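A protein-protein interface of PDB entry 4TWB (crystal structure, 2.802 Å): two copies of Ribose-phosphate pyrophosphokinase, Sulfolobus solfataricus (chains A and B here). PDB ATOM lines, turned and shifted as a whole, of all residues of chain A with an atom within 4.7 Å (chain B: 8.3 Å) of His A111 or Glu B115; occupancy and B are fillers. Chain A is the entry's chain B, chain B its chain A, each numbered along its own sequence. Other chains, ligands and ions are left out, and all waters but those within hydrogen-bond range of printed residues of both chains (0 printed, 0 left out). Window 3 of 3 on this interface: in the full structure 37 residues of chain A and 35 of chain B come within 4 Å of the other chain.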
ATOM      1  N   LYS A 107      21.386  18.530   9.626  1.00  0.00           N
ATOM      2  CA  LYS A 107      20.349  19.451   9.153  1.00  0.00           C
ATOM      3  C   LYS A 107      20.185  19.328   7.630  1.00  0.00           C
ATOM      4  O   LYS A 107      19.080  19.163   7.116  1.00  0.00           O
ATOM      5  CB  LYS A 107      20.675  20.894   9.556  1.00  0.00           C
ATOM      6  CG  LYS A 107      19.635  21.906   9.099  1.00  0.00           C
ATOM      7  CD  LYS A 107      19.861  23.275   9.735  1.00  0.00           C
ATOM      8  CE  LYS A 107      20.903  24.102   9.006  1.00  0.00           C
ATOM      9  NZ  LYS A 107      20.299  24.879   7.885  1.00  0.00           N
ATOM     10  N   THR A 108      21.309  19.377   6.928  1.00  0.00           N
ATOM     11  CA  THR A 108      21.340  19.265   5.479  1.00  0.00           C
ATOM     12  C   THR A 108      20.745  17.944   5.021  1.00  0.00           C
ATOM     13  O   THR A 108      19.904  17.897   4.127  1.00  0.00           O
ATOM     14  CB  THR A 108      22.786  19.344   4.959  1.00  0.00           C
ATOM     15  OG1 THR A 108      23.402  20.575   5.381  1.00  0.00           O
ATOM     16  CG2 THR A 108      22.783  19.267   3.467  1.00  0.00           C
ATOM     17  N   ILE A 109      21.197  16.862   5.634  1.00  0.00           N
ATOM     18  CA  ILE A 109      20.721  15.543   5.264  1.00  0.00           C
ATOM     19  C   ILE A 109      19.214  15.473   5.419  1.00  0.00           C
ATOM     20  O   ILE A 109      18.506  14.980   4.530  1.00  0.00           O
ATOM     21  CB  ILE A 109      21.312  14.462   6.165  1.00  0.00           C
ATOM     22  CG1 ILE A 109      22.839  14.435   6.069  1.00  0.00           C
ATOM     23  CG2 ILE A 109      20.737  13.126   5.794  1.00  0.00           C
ATOM     24  CD1 ILE A 109      23.346  13.925   4.744  1.00  0.00           C
ATOM     25  N   LEU A 110      18.724  15.971   6.553  1.00  0.00           N
ATOM     26  CA  LEU A 110      17.299  15.933   6.856  1.00  0.00           C
ATOM     27  C   LEU A 110      16.471  16.793   5.918  1.00  0.00           C
ATOM     28  O   LEU A 110      15.461  16.331   5.368  1.00  0.00           O
ATOM     29  CB  LEU A 110      17.044  16.342   8.305  1.00  0.00           C
ATOM     30  CG  LEU A 110      16.686  15.236   9.307  1.00  0.00           C
ATOM     31  CD1 LEU A 110      17.361  13.924   8.926  1.00  0.00           C
ATOM     32  CD2 LEU A 110      17.048  15.658  10.734  1.00  0.00           C
ATOM     33  N   HIS A 111      16.881  18.044   5.743  1.00  0.00           N
ATOM     34  CA  HIS A 111      16.239  18.897   4.751  1.00  0.00           C
ATOM     35  C   HIS A 111      16.159  18.222   3.379  1.00  0.00           C
ATOM     36  O   HIS A 111      15.112  18.291   2.714  1.00  0.00           O
ATOM     37  CB  HIS A 111      16.951  20.248   4.654  1.00  0.00           C
ATOM     38  CG  HIS A 111      16.665  21.150   5.813  1.00  0.00           C
ATOM     39  ND1 HIS A 111      17.515  22.162   6.205  1.00  0.00           N
ATOM     40  CD2 HIS A 111      15.622  21.179   6.677  1.00  0.00           C
ATOM     41  CE1 HIS A 111      17.003  22.781   7.253  1.00  0.00           C
ATOM     42  NE2 HIS A 111      15.855  22.203   7.560  1.00  0.00           N
ATOM     43  N   ILE A 112      17.256  17.574   2.968  1.00  0.00           N
ATOM     44  CA  ILE A 112      17.328  16.901   1.673  1.00  0.00           C
ATOM     45  C   ILE A 112      16.283  15.796   1.576  1.00  0.00           C
ATOM     46  O   ILE A 112      15.772  15.528   0.499  1.00  0.00           O
ATOM     47  CB  ILE A 112      18.729  16.295   1.411  1.00  0.00           C
ATOM     48  CG1 ILE A 112      19.736  17.381   1.073  1.00  0.00           C
ATOM     49  CG2 ILE A 112      18.697  15.298   0.279  1.00  0.00           C
ATOM     50  CD1 ILE A 112      21.080  16.843   0.637  1.00  0.00           C
ATOM     51  N   LEU A 113      15.974  15.141   2.691  1.00  0.00           N
ATOM     52  CA  LEU A 113      15.005  14.040   2.668  1.00  0.00           C
ATOM     53  C   LEU A 113      13.541  14.492   2.532  1.00  0.00           C
ATOM     54  O   LEU A 113      12.700  13.726   2.040  1.00  0.00           O
ATOM     55  CB  LEU A 113      15.138  13.169   3.917  1.00  0.00           C
ATOM     56  CG  LEU A 113      16.317  12.219   4.041  1.00  0.00           C
ATOM     57  CD1 LEU A 113      16.432  11.718   5.481  1.00  0.00           C
ATOM     58  CD2 LEU A 113      16.138  11.074   3.074  1.00  0.00           C
ATOM     59  N   SER A 114      13.230  15.708   3.003  1.00  0.00           N
ATOM     60  CA  SER A 114      11.895  16.307   2.832  1.00  0.00           C
ATOM     61  C   SER A 114      11.660  16.649   1.360  1.00  0.00           C
ATOM     62  O   SER A 114      10.731  16.139   0.728  1.00  0.00           O
ATOM     63  CB  SER A 114      11.748  17.579   3.676  1.00  0.00           C
ATOM     64  OG  SER A 114      11.916  17.308   5.057  1.00  0.00           O
ATOM     65  N   GLU A 115      12.500  17.537   0.831  1.00  0.00           N
ATOM     66  CA  GLU A 115      12.706  17.625  -0.607  1.00  0.00           C
ATOM     67  C   GLU A 115      13.075  16.194  -0.966  1.00  0.00           C
ATOM     68  O   GLU A 115      13.553  15.463  -0.097  1.00  0.00           O
ATOM     69  CB  GLU A 115      13.872  18.577  -0.895  1.00  0.00           C
ATOM     70  CG  GLU A 115      14.486  18.464  -2.288  1.00  0.00           C
ATOM     71  CD  GLU A 115      13.729  19.270  -3.326  1.00  0.00           C
ATOM     72  OE1 GLU A 115      12.950  20.170  -2.921  1.00  0.00           O
ATOM     73  OE2 GLU A 115      13.914  19.000  -4.542  1.00  0.00           O
ATOM     74  N   TYR A 134      14.647  18.982  12.566  1.00  0.00           N
ATOM     75  CA  TYR A 134      14.948  19.564  11.265  1.00  0.00           C
ATOM     76  C   TYR A 134      14.103  18.945  10.149  1.00  0.00           C
ATOM     77  O   TYR A 134      13.736  19.622   9.186  1.00  0.00           O
ATOM     78  CB  TYR A 134      16.433  19.408  10.959  1.00  0.00           C
ATOM     79  CG  TYR A 134      17.353  20.248  11.826  1.00  0.00           C
ATOM     80  CD1 TYR A 134      17.277  21.638  11.820  1.00  0.00           C
ATOM     81  CD2 TYR A 134      18.323  19.648  12.623  1.00  0.00           C
ATOM     82  CE1 TYR A 134      18.137  22.409  12.601  1.00  0.00           C
ATOM     83  CE2 TYR A 134      19.184  20.401  13.408  1.00  0.00           C
ATOM     84  CZ  TYR A 134      19.093  21.784  13.394  1.00  0.00           C
ATOM     85  OH  TYR A 134      19.956  22.542  14.173  1.00  0.00           O
ATOM     86  N   PHE B  68      26.892  19.521  -0.864  1.00  0.00           N
ATOM     87  CA  PHE B  68      25.636  19.846  -0.186  1.00  0.00           C
ATOM     88  C   PHE B  68      25.883  20.495   1.170  1.00  0.00           C
ATOM     89  O   PHE B  68      25.256  21.503   1.500  1.00  0.00           O
ATOM     90  CB  PHE B  68      24.768  18.612   0.031  1.00  0.00           C
ATOM     91  CG  PHE B  68      24.485  17.841  -1.209  1.00  0.00           C
ATOM     92  CD1 PHE B  68      24.395  18.470  -2.428  1.00  0.00           C
ATOM     93  CD2 PHE B  68      24.283  16.475  -1.147  1.00  0.00           C
ATOM     94  CE1 PHE B  68      24.121  17.755  -3.573  1.00  0.00           C
ATOM     95  CE2 PHE B  68      24.011  15.753  -2.283  1.00  0.00           C
ATOM     96  CZ  PHE B  68      23.929  16.398  -3.505  1.00  0.00           C
ATOM     97  N   ALA B  71      27.550  23.963   0.902  1.00  0.00           N
ATOM     98  CA  ALA B  71      26.592  24.910   0.363  1.00  0.00           C
ATOM     99  C   ALA B  71      25.651  25.458   1.435  1.00  0.00           C
ATOM    100  O   ALA B  71      25.540  26.669   1.599  1.00  0.00           O
ATOM    101  CB  ALA B  71      25.808  24.278  -0.753  1.00  0.00           C
ATOM    102  N   GLU B  72      24.975  24.575   2.165  1.00  0.00           N
ATOM    103  CA  GLU B  72      24.081  25.019   3.242  1.00  0.00           C
ATOM    104  C   GLU B  72      24.804  25.837   4.311  1.00  0.00           C
ATOM    105  O   GLU B  72      24.306  26.870   4.740  1.00  0.00           O
ATOM    106  CB  GLU B  72      23.326  23.852   3.879  1.00  0.00           C
ATOM    107  CG  GLU B  72      21.907  23.702   3.354  1.00  0.00           C
ATOM    108  CD  GLU B  72      20.952  23.174   4.403  1.00  0.00           C
ATOM    109  OE1 GLU B  72      21.430  22.661   5.438  1.00  0.00           O
ATOM    110  OE2 GLU B  72      19.722  23.278   4.198  1.00  0.00           O
ATOM    111  N   ARG B  75      25.225  29.362   2.990  1.00  0.00           N
ATOM    112  CA  ARG B  75      23.980  30.118   3.034  1.00  0.00           C
ATOM    113  C   ARG B  75      23.630  30.461   4.482  1.00  0.00           C
ATOM    114  O   ARG B  75      23.132  31.551   4.772  1.00  0.00           O
ATOM    115  CB  ARG B  75      22.837  29.343   2.367  1.00  0.00           C
ATOM    116  CG  ARG B  75      21.496  30.060   2.447  1.00  0.00           C
ATOM    117  CD  ARG B  75      20.349  29.144   2.055  1.00  0.00           C
ATOM    118  NE  ARG B  75      20.196  28.031   2.990  1.00  0.00           N
ATOM    119  CZ  ARG B  75      19.447  26.954   2.759  1.00  0.00           C
ATOM    120  NH1 ARG B  75      18.776  26.840   1.612  1.00  0.00           N
ATOM    121  NH2 ARG B  75      19.371  25.991   3.674  1.00  0.00           N
ATOM    122  N   ASP B  76      23.912  29.523   5.386  1.00  0.00           N
ATOM    123  CA  ASP B  76      23.620  29.694   6.808  1.00  0.00           C
ATOM    124  C   ASP B  76      24.500  30.774   7.419  1.00  0.00           C
ATOM    125  O   ASP B  76      24.105  31.436   8.375  1.00  0.00           O
ATOM    126  CB  ASP B  76      23.844  28.384   7.581  1.00  0.00           C
ATOM    127  CG  ASP B  76      22.697  27.389   7.422  1.00  0.00           C
ATOM    128  OD1 ASP B  76      21.672  27.720   6.770  1.00  0.00           O
ATOM    129  OD2 ASP B  76      22.839  26.263   7.958  1.00  0.00           O
ATOM    130  N   LEU B  82      25.241  32.578  -3.629  1.00  0.00           N
ATOM    131  CA  LEU B  82      26.097  31.412  -3.751  1.00  0.00           C
ATOM    132  C   LEU B  82      26.184  31.039  -5.222  1.00  0.00           C
ATOM    133  O   LEU B  82      25.165  30.764  -5.866  1.00  0.00           O
ATOM    134  CB  LEU B  82      25.544  30.227  -2.954  1.00  0.00           C
ATOM    135  CG  LEU B  82      26.571  29.256  -2.369  1.00  0.00           C
ATOM    136  CD1 LEU B  82      26.039  27.836  -2.482  1.00  0.00           C
ATOM    137  CD2 LEU B  82      27.948  29.373  -3.023  1.00  0.00           C
ATOM    138  N   THR B 108      17.633  14.687  -9.524  1.00  0.00           N
ATOM    139  CA  THR B 108      17.710  14.682  -8.074  1.00  0.00           C
ATOM    140  C   THR B 108      18.868  15.542  -7.578  1.00  0.00           C
ATOM    141  O   THR B 108      18.703  16.371  -6.682  1.00  0.00           O
ATOM    142  CB  THR B 108      17.898  13.261  -7.545  1.00  0.00           C
ATOM    143  OG1 THR B 108      16.810  12.437  -7.976  1.00  0.00           O
ATOM    144  CG2 THR B 108      17.952  13.257  -6.021  1.00  0.00           C
ATOM    145  N   ILE B 109      20.044  15.339  -8.155  1.00  0.00           N
ATOM    146  CA  ILE B 109      21.205  16.109  -7.765  1.00  0.00           C
ATOM    147  C   ILE B 109      20.928  17.593  -7.926  1.00  0.00           C
ATOM    148  O   ILE B 109      21.211  18.390  -7.028  1.00  0.00           O
ATOM    149  CB  ILE B 109      22.410  15.746  -8.630  1.00  0.00           C
ATOM    150  CG1 ILE B 109      22.684  14.252  -8.549  1.00  0.00           C
ATOM    151  CG2 ILE B 109      23.633  16.543  -8.201  1.00  0.00           C
ATOM    152  CD1 ILE B 109      23.330  13.864  -7.262  1.00  0.00           C
ATOM    153  N   LEU B 110      20.375  17.961  -9.078  1.00  0.00           N
ATOM    154  CA  LEU B 110      20.130  19.372  -9.397  1.00  0.00           C
ATOM    155  C   LEU B 110      19.094  19.979  -8.459  1.00  0.00           C
ATOM    156  O   LEU B 110      19.286  21.068  -7.912  1.00  0.00           O
ATOM    157  CB  LEU B 110      19.704  19.544 -10.863  1.00  0.00           C
ATOM    158  CG  LEU B 110      20.730  20.125 -11.835  1.00  0.00           C
ATOM    159  CD1 LEU B 110      22.128  19.715 -11.453  1.00  0.00           C
ATOM    160  CD2 LEU B 110      20.419  19.704 -13.258  1.00  0.00           C
ATOM    161  N   HIS B 111      17.991  19.268  -8.266  1.00  0.00           N
ATOM    162  CA  HIS B 111      16.969  19.740  -7.345  1.00  0.00           C
ATOM    163  C   HIS B 111      17.568  19.958  -5.966  1.00  0.00           C
ATOM    164  O   HIS B 111      17.264  20.935  -5.298  1.00  0.00           O
ATOM    165  CB  HIS B 111      15.796  18.762  -7.291  1.00  0.00           C
ATOM    166  CG  HIS B 111      14.872  18.863  -8.469  1.00  0.00           C
ATOM    167  ND1 HIS B 111      14.072  17.819  -8.882  1.00  0.00           N
ATOM    168  CD2 HIS B 111      14.631  19.885  -9.328  1.00  0.00           C
ATOM    169  CE1 HIS B 111      13.370  18.196  -9.940  1.00  0.00           C
ATOM    170  NE2 HIS B 111      13.692  19.444 -10.231  1.00  0.00           N
ATOM    171  N   ILE B 112      18.436  19.046  -5.549  1.00  0.00           N
ATOM    172  CA  ILE B 112      19.087  19.153  -4.252  1.00  0.00           C
ATOM    173  C   ILE B 112      19.936  20.403  -4.129  1.00  0.00           C
ATOM    174  O   ILE B 112      20.048  20.954  -3.041  1.00  0.00           O
ATOM    175  CB  ILE B 112      19.983  17.930  -3.954  1.00  0.00           C
ATOM    176  CG1 ILE B 112      19.125  16.701  -3.633  1.00  0.00           C
ATOM    177  CG2 ILE B 112      20.948  18.220  -2.803  1.00  0.00           C
ATOM    178  CD1 ILE B 112      19.920  15.496  -3.181  1.00  0.00           C
ATOM    179  N   LEU B 113      20.558  20.832  -5.227  1.00  0.00           N
ATOM    180  CA  LEU B 113      21.413  22.021  -5.203  1.00  0.00           C
ATOM    181  C   LEU B 113      20.632  23.328  -5.075  1.00  0.00           C
ATOM    182  O   LEU B 113      21.158  24.305  -4.553  1.00  0.00           O
ATOM    183  CB  LEU B 113      22.299  22.084  -6.445  1.00  0.00           C
ATOM    184  CG  LEU B 113      23.476  21.117  -6.529  1.00  0.00           C
ATOM    185  CD1 LEU B 113      24.050  21.116  -7.939  1.00  0.00           C
ATOM    186  CD2 LEU B 113      24.551  21.498  -5.537  1.00  0.00           C
ATOM    187  N   SER B 114      19.396  23.358  -5.575  1.00  0.00           N
ATOM    188  CA  SER B 114      18.538  24.544  -5.447  1.00  0.00           C
ATOM    189  C   SER B 114      18.127  24.722  -3.988  1.00  0.00           C
ATOM    190  O   SER B 114      18.418  25.753  -3.373  1.00  0.00           O
ATOM    191  CB  SER B 114      17.290  24.440  -6.333  1.00  0.00           C
ATOM    192  OG  SER B 114      17.615  24.301  -7.706  1.00  0.00           O
ATOM    193  N   GLU B 115      17.424  23.719  -3.454  1.00  0.00           N
ATOM    194  CA  GLU B 115      17.343  23.507  -2.013  1.00  0.00           C
ATOM    195  C   GLU B 115      18.809  23.459  -1.630  1.00  0.00           C
ATOM    196  O   GLU B 115      19.629  23.125  -2.471  1.00  0.00           O
ATOM    197  CB  GLU B 115      16.660  22.165  -1.746  1.00  0.00           C
ATOM    198  CG  GLU B 115      16.859  21.588  -0.349  1.00  0.00           C
ATOM    199  CD  GLU B 115      15.896  22.173   0.673  1.00  0.00           C
ATOM    200  OE1 GLU B 115      14.866  22.756   0.254  1.00  0.00           O
ATOM    201  OE2 GLU B 115      16.170  22.045   1.893  1.00  0.00           O
ATOM    202  N   VAL B 116      19.175  23.813  -0.409  1.00  0.00           N
ATOM    203  CA  VAL B 116      20.601  23.813  -0.042  1.00  0.00           C
ATOM    204  C   VAL B 116      21.275  25.148  -0.336  1.00  0.00           C
ATOM    205  O   VAL B 116      22.304  25.471   0.262  1.00  0.00           O
ATOM    206  CB  VAL B 116      21.401  22.646  -0.697  1.00  0.00           C
ATOM    207  CG1 VAL B 116      22.777  23.095  -1.127  1.00  0.00           C
ATOM    208  CG2 VAL B 116      21.514  21.457   0.236  1.00  0.00           C
ATOM    209  N   GLY B 117      20.697  25.918  -1.258  1.00  0.00           N
ATOM    210  CA  GLY B 117      21.021  27.337  -1.394  1.00  0.00           C
ATOM    211  C   GLY B 117      21.901  27.834  -2.539  1.00  0.00           C
ATOM    212  O   GLY B 117      22.344  28.987  -2.513  1.00  0.00           O
ATOM    213  N   VAL B 118      22.171  26.992  -3.536  1.00  0.00           N
ATOM    214  CA  VAL B 118      22.951  27.426  -4.696  1.00  0.00           C
ATOM    215  C   VAL B 118      22.097  28.305  -5.617  1.00  0.00           C
ATOM    216  O   VAL B 118      21.021  27.905  -6.079  1.00  0.00           O
ATOM    217  CB  VAL B 118      23.523  26.232  -5.490  1.00  0.00           C
ATOM    218  CG1 VAL B 118      24.268  26.726  -6.694  1.00  0.00           C
ATOM    219  CG2 VAL B 118      24.442  25.402  -4.620  1.00  0.00           C
ATOM    220  N   ASN B 119      22.584  29.512  -5.877  1.00  0.00           N
ATOM    221  CA  ASN B 119      21.854  30.464  -6.705  1.00  0.00           C
ATOM    222  C   ASN B 119      22.220  30.302  -8.169  1.00  0.00           C
ATOM    223  O   ASN B 119      21.358  30.247  -9.053  1.00  0.00           O
ATOM    224  CB  ASN B 119      22.170  31.896  -6.271  1.00  0.00           C
ATOM    225  CG  ASN B 119      21.675  32.206  -4.875  1.00  0.00           C
ATOM    226  OD1 ASN B 119      22.455  32.541  -3.977  1.00  0.00           O
ATOM    227  ND2 ASN B 119      20.371  32.086  -4.682  1.00  0.00           N
ATOM    228  N   PHE B 135      17.748  22.411 -12.915  1.00  0.00           N
ATOM    229  CA  PHE B 135      18.229  23.356 -11.906  1.00  0.00           C
ATOM    230  C   PHE B 135      17.444  24.655 -12.017  1.00  0.00           C
ATOM    231  O   PHE B 135      17.296  25.210 -13.109  1.00  0.00           O
ATOM    232  CB  PHE B 135      19.717  23.621 -12.071  1.00  0.00           C
ATOM    233  CG  PHE B 135      20.272  24.613 -11.088  1.00  0.00           C
ATOM    234  CD1 PHE B 135      20.427  24.278  -9.753  1.00  0.00           C
ATOM    235  CD2 PHE B 135      20.663  25.873 -11.502  1.00  0.00           C
ATOM    236  CE1 PHE B 135      20.957  25.180  -8.844  1.00  0.00           C
ATOM    237  CE2 PHE B 135      21.195  26.782 -10.609  1.00  0.00           C
ATOM    238  CZ  PHE B 135      21.340  26.434  -9.273  1.00  0.00           C
ATOM    239  N   LYS B 136      16.940  25.132 -10.879  1.00  0.00           N
ATOM    240  CA  LYS B 136      16.006  26.252 -10.869  1.00  0.00           C
ATOM    241  C   LYS B 136      16.671  27.630 -10.946  1.00  0.00           C
ATOM    242  O   LYS B 136      16.112  28.559 -11.533  1.00  0.00           O
ATOM    243  CB  LYS B 136      15.048  26.144  -9.678  1.00  0.00           C
ATOM    244  CG  LYS B 136      14.023  25.025  -9.845  1.00  0.00           C
ATOM    245  CD  LYS B 136      13.370  25.090 -11.237  1.00  0.00           C
ATOM    246  CE  LYS B 136      12.631  23.799 -11.600  1.00  0.00           C
ATOM    247  NZ  LYS B 136      12.252  23.742 -13.051  1.00  0.00           N
ATOM    248  N   GLY B 137      17.865  27.759 -10.377  1.00  0.00           N
ATOM    249  CA  GLY B 137      18.610  29.003 -10.459  1.00  0.00           C
ATOM    250  C   GLY B 137      19.159  29.352 -11.834  1.00  0.00           C
ATOM    251  O   GLY B 137      18.660  28.885 -12.866  1.00  0.00           O
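The guanidinium group (NH2) of Arg B75 lies within salt-bridge range of the side-chain carboxylate (OE2) of Glu B72, 2.8 Å away.
N of Glu B72 sits at hydrogen-bond distance from O of Val B116 (3.4 Å).
His A111 touches Glu B115, and with the chains exchanged Glu A115 touches His B111.
Ile A112 touches its own counterpart, Ile B112.
Among the printed residues, merely in contact across the chains: Glu A115 with His B111, His A111 with Glu B115, Ile A112 with Ile B112, Ile A112 with Phe B68 and Thr A108 with Phe B68.
Of chain B, only Glu B72 (3.2 Å) and Glu B115 (3.4 Å) come within 4 Å of His A111.
Glu B115 touches just one residue of chain A: His A111.
Of the printed residues of chain A, His B111 touches Glu A115 (3.3 Å).
Of the printed residues of chain A, Ile B112 touches Ile A112.
Printed residues of chain A within 4 Å of Phe B68: Thr A108 and Ile A112.
The nearest residue of chain A that does not touch Glu B115 is Glu A115 (4.3 Å).
Hydrophobic or aromatic side chains of chain A within 4 Å of the printed part of chain B: His A111 and Ile A112.
Among the printed residues, 9 pairs touch across the chains.
OE1 of Glu B72 is in salt-bridge range of NZ of Lys A107.
OE1 of Glu B72 is in hydrogen-bond range of OG1 of Thr A108 (2.9 Å).
The side-chain carboxylate of Glu B72 is in hydrogen-bond range of a ring nitrogen (ND1) of His A111 (3.2 Å).
NZ of Lys A107 is in salt-bridge range of OD2 of Asp B76, 2.9 Å away.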
